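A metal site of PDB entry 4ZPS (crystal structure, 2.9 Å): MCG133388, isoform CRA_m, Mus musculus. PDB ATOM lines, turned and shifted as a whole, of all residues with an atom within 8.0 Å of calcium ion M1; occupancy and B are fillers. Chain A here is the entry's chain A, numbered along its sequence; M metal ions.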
ATOM      1  N   ASP A  96      14.793   3.418  12.204  1.00  0.00           N
ATOM      2  CA  ASP A  96      15.876   2.494  12.520  1.00  0.00           C
ATOM      3  C   ASP A  96      16.504   2.831  13.859  1.00  0.00           C
ATOM      4  O   ASP A  96      16.794   3.996  14.146  1.00  0.00           O
ATOM      5  CB  ASP A  96      16.944   2.526  11.407  1.00  0.00           C
ATOM      6  CG  ASP A  96      18.117   1.606  11.695  1.00  0.00           C
ATOM      7  OD1 ASP A  96      19.058   2.028  12.400  1.00  0.00           O
ATOM      8  OD2 ASP A  96      18.113   0.463  11.198  1.00  0.00           O
ATOM      9  N   ILE A  97      16.704   1.815  14.685  1.00  0.00           N
ATOM     10  CA  ILE A  97      17.376   1.984  15.974  1.00  0.00           C
ATOM     11  C   ILE A  97      18.654   1.159  15.997  1.00  0.00           C
ATOM     12  O   ILE A  97      18.853   0.281  15.154  1.00  0.00           O
ATOM     13  CB  ILE A  97      16.471   1.578  17.144  1.00  0.00           C
ATOM     14  N   ASN A  98      19.524   1.439  16.965  1.00  0.00           N
ATOM     15  CA  ASN A  98      20.790   0.726  17.078  1.00  0.00           C
ATOM     16  C   ASN A  98      20.680  -0.502  17.970  1.00  0.00           C
ATOM     17  O   ASN A  98      20.802  -0.408  19.187  1.00  0.00           O
ATOM     18  CB  ASN A  98      21.876   1.657  17.608  1.00  0.00           C
ATOM     19  CG  ASN A  98      23.271   1.176  17.286  1.00  0.00           C
ATOM     20  OD1 ASN A  98      23.484  -0.001  16.998  1.00  0.00           O
ATOM     21  ND2 ASN A  98      24.242   2.081  17.322  1.00  0.00           N
ATOM     22  N   ASP A  99      20.428  -1.653  17.350  1.00  0.00           N
ATOM     23  CA  ASP A  99      20.338  -2.918  18.089  1.00  0.00           C
ATOM     24  C   ASP A  99      21.142  -4.004  17.393  1.00  0.00           C
ATOM     25  O   ASP A  99      21.057  -5.184  17.752  1.00  0.00           O
ATOM     26  CB  ASP A  99      18.881  -3.346  18.244  1.00  0.00           C
ATOM     27  CG  ASP A  99      18.188  -3.540  16.903  1.00  0.00           C
ATOM     28  OD1 ASP A  99      18.467  -2.775  15.960  1.00  0.00           O
ATOM     29  OD2 ASP A  99      17.368  -4.477  16.796  1.00  0.00           O
ATOM     30  N   ASN A 100      21.912  -3.602  16.380  1.00  0.00           N
ATOM     31  CA  ASN A 100      22.722  -4.551  15.619  1.00  0.00           C
ATOM     32  C   ASN A 100      24.085  -3.966  15.248  1.00  0.00           C
ATOM     33  O   ASN A 100      24.255  -3.363  14.190  1.00  0.00           O
ATOM     34  CB  ASN A 100      21.971  -4.975  14.356  1.00  0.00           C
ATOM     35  N   ASN A 101      25.047  -4.155  16.140  1.00  0.00           N
ATOM     36  CA  ASN A 101      26.419  -3.693  15.937  1.00  0.00           C
ATOM     37  C   ASN A 101      27.098  -4.408  14.764  1.00  0.00           C
ATOM     38  O   ASN A 101      26.665  -5.490  14.352  1.00  0.00           O
ATOM     39  CB  ASN A 101      27.233  -3.904  17.215  1.00  0.00           C
ATOM     40  CG  ASN A 101      26.990  -5.262  17.832  1.00  0.00           C
ATOM     41  OD1 ASN A 101      26.328  -6.119  17.238  1.00  0.00           O
ATOM     42  ND2 ASN A 101      27.517  -5.467  19.033  1.00  0.00           N
ATOM     43  N   PRO A 102      28.148  -3.794  14.197  1.00  0.00           N
ATOM     44  CA  PRO A 102      28.930  -4.434  13.130  1.00  0.00           C
ATOM     45  C   PRO A 102      29.606  -5.706  13.617  1.00  0.00           C
ATOM     46  O   PRO A 102      30.540  -5.636  14.415  1.00  0.00           O
ATOM     47  CB  PRO A 102      29.980  -3.372  12.774  1.00  0.00           C
ATOM     48  CG  PRO A 102      29.397  -2.085  13.236  1.00  0.00           C
ATOM     49  CD  PRO A 102      28.616  -2.424  14.460  1.00  0.00           C
ATOM     50  N   LYS A 103      29.147  -6.852  13.138  1.00  0.00           N
ATOM     51  CA  LYS A 103      29.705  -8.134  13.571  1.00  0.00           C
ATOM     52  C   LYS A 103      30.526  -8.784  12.471  1.00  0.00           C
ATOM     53  O   LYS A 103      30.091  -8.867  11.326  1.00  0.00           O
ATOM     54  CB  LYS A 103      28.585  -9.079  14.027  1.00  0.00           C
ATOM     55  N   VAL A 129      29.819  -6.861   9.093  1.00  0.00           N
ATOM     56  CA  VAL A 129      28.584  -6.425   8.452  1.00  0.00           C
ATOM     57  C   VAL A 129      27.711  -5.629   9.420  1.00  0.00           C
ATOM     58  O   VAL A 129      27.596  -5.972  10.601  1.00  0.00           O
ATOM     59  CB  VAL A 129      27.773  -7.617   7.907  1.00  0.00           C
ATOM     60  CG1 VAL A 129      28.303  -8.040   6.552  1.00  0.00           C
ATOM     61  CG2 VAL A 129      27.790  -8.768   8.903  1.00  0.00           C
ATOM     62  N   ASP A 130      27.098  -4.560   8.913  1.00  0.00           N
ATOM     63  CA  ASP A 130      26.206  -3.730   9.712  1.00  0.00           C
ATOM     64  C   ASP A 130      24.768  -3.856   9.235  1.00  0.00           C
ATOM     65  O   ASP A 130      24.381  -3.279   8.224  1.00  0.00           O
ATOM     66  CB  ASP A 130      26.654  -2.271   9.653  1.00  0.00           C
ATOM     67  CG  ASP A 130      26.988  -1.815   8.251  1.00  0.00           C
ATOM     68  OD1 ASP A 130      28.112  -2.093   7.777  1.00  0.00           O
ATOM     69  OD2 ASP A 130      26.125  -1.173   7.603  1.00  0.00           O
ATOM     70  N   PRO A 131      23.954  -4.644   9.971  1.00  0.00           N
ATOM     71  CA  PRO A 131      22.539  -4.831   9.643  1.00  0.00           C
ATOM     72  C   PRO A 131      21.794  -3.511   9.554  1.00  0.00           C
ATOM     73  O   PRO A 131      20.960  -3.322   8.660  1.00  0.00           O
ATOM     74  CB  PRO A 131      22.018  -5.686  10.804  1.00  0.00           C
ATOM     75  CG  PRO A 131      23.226  -6.406  11.302  1.00  0.00           C
ATOM     76  CD  PRO A 131      24.363  -5.432  11.148  1.00  0.00           C
ATOM     77  N   ASP A 132      22.088  -2.599  10.476  1.00  0.00           N
ATOM     78  CA  ASP A 132      21.522  -1.259  10.448  1.00  0.00           C
ATOM     79  C   ASP A 132      22.272  -0.405   9.422  1.00  0.00           C
ATOM     80  O   ASP A 132      23.443  -0.671   9.144  1.00  0.00           O
ATOM     81  CB  ASP A 132      21.572  -0.615  11.823  1.00  0.00           C
ATOM     82  CG  ASP A 132      21.328  -1.602  12.945  1.00  0.00           C
ATOM     83  OD1 ASP A 132      20.567  -2.576  12.725  1.00  0.00           O
ATOM     84  OD2 ASP A 132      21.897  -1.422  14.033  1.00  0.00           O
ATOM     85  N   VAL A 133      21.601   0.598   8.878  1.00  0.00           N
ATOM     86  CA  VAL A 133      22.222   1.462   7.879  1.00  0.00           C
ATOM     87  C   VAL A 133      22.122   2.929   8.304  1.00  0.00           C
ATOM     88  O   VAL A 133      21.105   3.354   8.875  1.00  0.00           O
ATOM     89  CB  VAL A 133      21.564   1.291   6.492  1.00  0.00           C
ATOM     90  CG1 VAL A 133      22.335   2.058   5.433  1.00  0.00           C
ATOM     91  CG2 VAL A 133      21.484  -0.184   6.123  1.00  0.00           C
ATOM     92  N   ILE A 135      23.936   6.212  10.417  1.00  0.00           N
ATOM     93  CA  ILE A 135      24.835   6.484  11.520  1.00  0.00           C
ATOM     94  C   ILE A 135      24.955   5.248  12.396  1.00  0.00           C
ATOM     95  O   ILE A 135      25.994   5.003  13.016  1.00  0.00           O
ATOM     96  CB  ILE A 135      24.374   7.702  12.355  1.00  0.00           C
ATOM     97  CG1 ILE A 135      25.410   8.069  13.425  1.00  0.00           C
ATOM     98  CG2 ILE A 135      23.015   7.443  12.988  1.00  0.00           C
ATOM     99  CD1 ILE A 135      26.777   8.399  12.854  1.00  0.00           C
ATOM    100  N   ASN A 136      23.901   4.437  12.423  1.00  0.00           N
ATOM    101  CA  ASN A 136      23.878   3.204  13.191  1.00  0.00           C
ATOM    102  C   ASN A 136      24.453   2.034  12.411  1.00  0.00           C
ATOM    103  O   ASN A 136      24.156   0.877  12.697  1.00  0.00           O
ATOM    104  CB  ASN A 136      22.453   2.882  13.648  1.00  0.00           C
ATOM    105  CG  ASN A 136      21.829   4.007  14.437  1.00  0.00           C
ATOM    106  OD1 ASN A 136      22.087   4.171  15.624  1.00  0.00           O
ATOM    107  ND2 ASN A 136      20.981   4.783  13.773  1.00  0.00           N
ATOM    108  N   SER A 137      25.277   2.348  11.415  1.00  0.00           N
ATOM    109  CA  SER A 137      25.970   1.338  10.627  1.00  0.00           C
ATOM    110  C   SER A 137      27.457   1.363  10.942  1.00  0.00           C
ATOM    111  O   SER A 137      27.906   2.164  11.756  1.00  0.00           O
ATOM    112  CB  SER A 137      25.734   1.557   9.136  1.00  0.00           C
ATOM    113  OG  SER A 137      26.233   2.821   8.723  1.00  0.00           O
ATOM    114  N   LEU A 138      28.226   0.486  10.302  1.00  0.00           N
ATOM    115  CA  LEU A 138      29.668   0.433  10.501  1.00  0.00           C
ATOM    116  C   LEU A 138      30.301   1.784  10.189  1.00  0.00           C
ATOM    117  O   LEU A 138      30.115   2.328   9.093  1.00  0.00           O
ATOM    118  CB  LEU A 138      30.301  -0.662   9.647  1.00  0.00           C
ATOM    119  N   SER A 186      33.790  -0.319  14.696  1.00  0.00           N
ATOM    120  CA  SER A 186      32.984   0.548  15.545  1.00  0.00           C
ATOM    121  C   SER A 186      31.837   1.240  14.802  1.00  0.00           C
ATOM    122  O   SER A 186      31.926   1.522  13.599  1.00  0.00           O
ATOM    123  CB  SER A 186      33.871   1.607  16.204  1.00  0.00           C
ATOM    124  OG  SER A 186      34.814   1.010  17.074  1.00  0.00           O
ATOM    125  N   ASP A 187      30.794   1.530  15.567  1.00  0.00           N
ATOM    126  CA  ASP A 187      29.516   2.049  15.073  1.00  0.00           C
ATOM    127  C   ASP A 187      29.093   3.263  15.888  1.00  0.00           C
ATOM    128  O   ASP A 187      29.180   3.253  17.123  1.00  0.00           O
ATOM    129  CB  ASP A 187      28.450   0.958  15.171  1.00  0.00           C
ATOM    130  CG  ASP A 187      27.158   1.313  14.454  1.00  0.00           C
ATOM    131  OD1 ASP A 187      26.817   2.517  14.364  1.00  0.00           O
ATOM    132  OD2 ASP A 187      26.487   0.386  13.981  1.00  0.00           O
ATOM    133  N   GLY A 188      28.608   4.290  15.205  1.00  0.00           N
ATOM    134  CA  GLY A 188      28.178   5.520  15.852  1.00  0.00           C
ATOM    135  C   GLY A 188      26.763   5.450  16.411  1.00  0.00           C
ATOM    136  O   GLY A 188      25.792   5.610  15.676  1.00  0.00           O
ATOM    137  N   GLY A 189      26.657   5.208  17.711  1.00  0.00           N
ATOM    138  CA  GLY A 189      25.375   5.162  18.383  1.00  0.00           C
ATOM    139  C   GLY A 189      25.458   5.764  19.769  1.00  0.00           C
ATOM    140  O   GLY A 189      26.369   6.525  20.062  1.00  0.00           O
ATOM    141  N   PRO A 191      25.283   4.124  23.499  1.00  0.00           N
ATOM    142  CA  PRO A 191      26.681   4.461  23.219  1.00  0.00           C
ATOM    143  C   PRO A 191      27.167   3.875  21.891  1.00  0.00           C
ATOM    144  O   PRO A 191      26.422   3.141  21.234  1.00  0.00           O
ATOM    145  CB  PRO A 191      27.431   3.820  24.390  1.00  0.00           C
ATOM    146  CG  PRO A 191      26.609   2.626  24.719  1.00  0.00           C
ATOM    147  CD  PRO A 191      25.174   3.037  24.486  1.00  0.00           C
ATOM    148  N   ARG A 192      28.394   4.203  21.499  1.00  0.00           N
ATOM    149  CA  ARG A 192      28.966   3.694  20.258  1.00  0.00           C
ATOM    150  C   ARG A 192      29.091   2.173  20.294  1.00  0.00           C
ATOM    151  O   ARG A 192      29.764   1.609  21.161  1.00  0.00           O
ATOM    152  CB  ARG A 192      30.333   4.319  19.994  1.00  0.00           C
ATOM    153  CG  ARG A 192      30.276   5.715  19.408  1.00  0.00           C
ATOM    154  CD  ARG A 192      31.654   6.171  18.953  1.00  0.00           C
ATOM    155  NE  ARG A 192      31.613   7.463  18.280  1.00  0.00           N
ATOM    156  CZ  ARG A 192      32.673   8.081  17.766  1.00  0.00           C
ATOM    157  NH1 ARG A 192      33.869   7.530  17.847  1.00  0.00           N
ATOM    158  NH2 ARG A 192      32.533   9.264  17.173  1.00  0.00           N
ATOM    159  N   ARG A 193      28.434   1.507  19.344  1.00  0.00           N
ATOM    160  CA  ARG A 193      28.516   0.052  19.235  1.00  0.00           C
ATOM    161  C   ARG A 193      29.891  -0.355  18.735  1.00  0.00           C
ATOM    162  O   ARG A 193      30.634   0.477  18.224  1.00  0.00           O
ATOM    163  CB  ARG A 193      27.446  -0.472  18.291  1.00  0.00           C
ATOM    164  CG  ARG A 193      26.040  -0.436  18.845  1.00  0.00           C
ATOM    165  CD  ARG A 193      25.848  -1.480  19.924  1.00  0.00           C
ATOM    166  NE  ARG A 193      24.430  -1.736  20.178  1.00  0.00           N
ATOM    167  CZ  ARG A 193      23.979  -2.624  21.049  1.00  0.00           C
ATOM    168  NH1 ARG A 193      24.830  -3.345  21.768  1.00  0.00           N
ATOM    169  NH2 ARG A 193      22.666  -2.789  21.209  1.00  0.00           N
ATOM    170  N   SER A 194      30.233  -1.634  18.903  1.00  0.00           N
ATOM    171  CA  SER A 194      31.491  -2.172  18.375  1.00  0.00           C
ATOM    172  C   SER A 194      31.634  -3.670  18.564  1.00  0.00           C
ATOM    173  O   SER A 194      31.092  -4.245  19.514  1.00  0.00           O
ATOM    174  CB  SER A 194      32.704  -1.482  19.004  1.00  0.00           C
ATOM    175  OG  SER A 194      32.744  -1.707  20.397  1.00  0.00           O
HETATM  176 CA    CA M   1      24.615  -1.029  14.943  1.00  0.00          CA
HETATM  177 CA    CA M   2      17.904  -0.947  13.128  1.00  0.00          CA
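The side-chain carboxylate of Asp 187 sits close to the backbone carbonyl oxygen of Asn 136 (2.7 Å). ND2 of Asn 98 sits close to OD1 of Asn 136, 3.4 Å away. OD1 of Asp 187 is in hydrogen-bond range of N of Ser 137, 3.3 Å away. The backbone NH (N) of Asp 187 lies within hydrogen-bond range of the backbone carbonyl oxygen (O) of Arg 193.
Asn 101 touches calcium ion M1 (CA to CA, 3.4 Å). The nearest printed residue that does not touch calcium ion M1 is Arg 193 (4.2 Å).
Calcium ion M1 is bound by the backbone carbonyl oxygen of Asn 100 (2.5 Å), the side-chain carboxylate of Asp 187 (2.5 Å), the side-chain amide oxygen of Asn 98 (2.6 Å) and the side-chain carboxylate of Asp 132 (2.9 Å). Slightly farther from calcium ion M1 lies the backbone carbonyl oxygen (O) of Asn 136 (3.0 Å).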
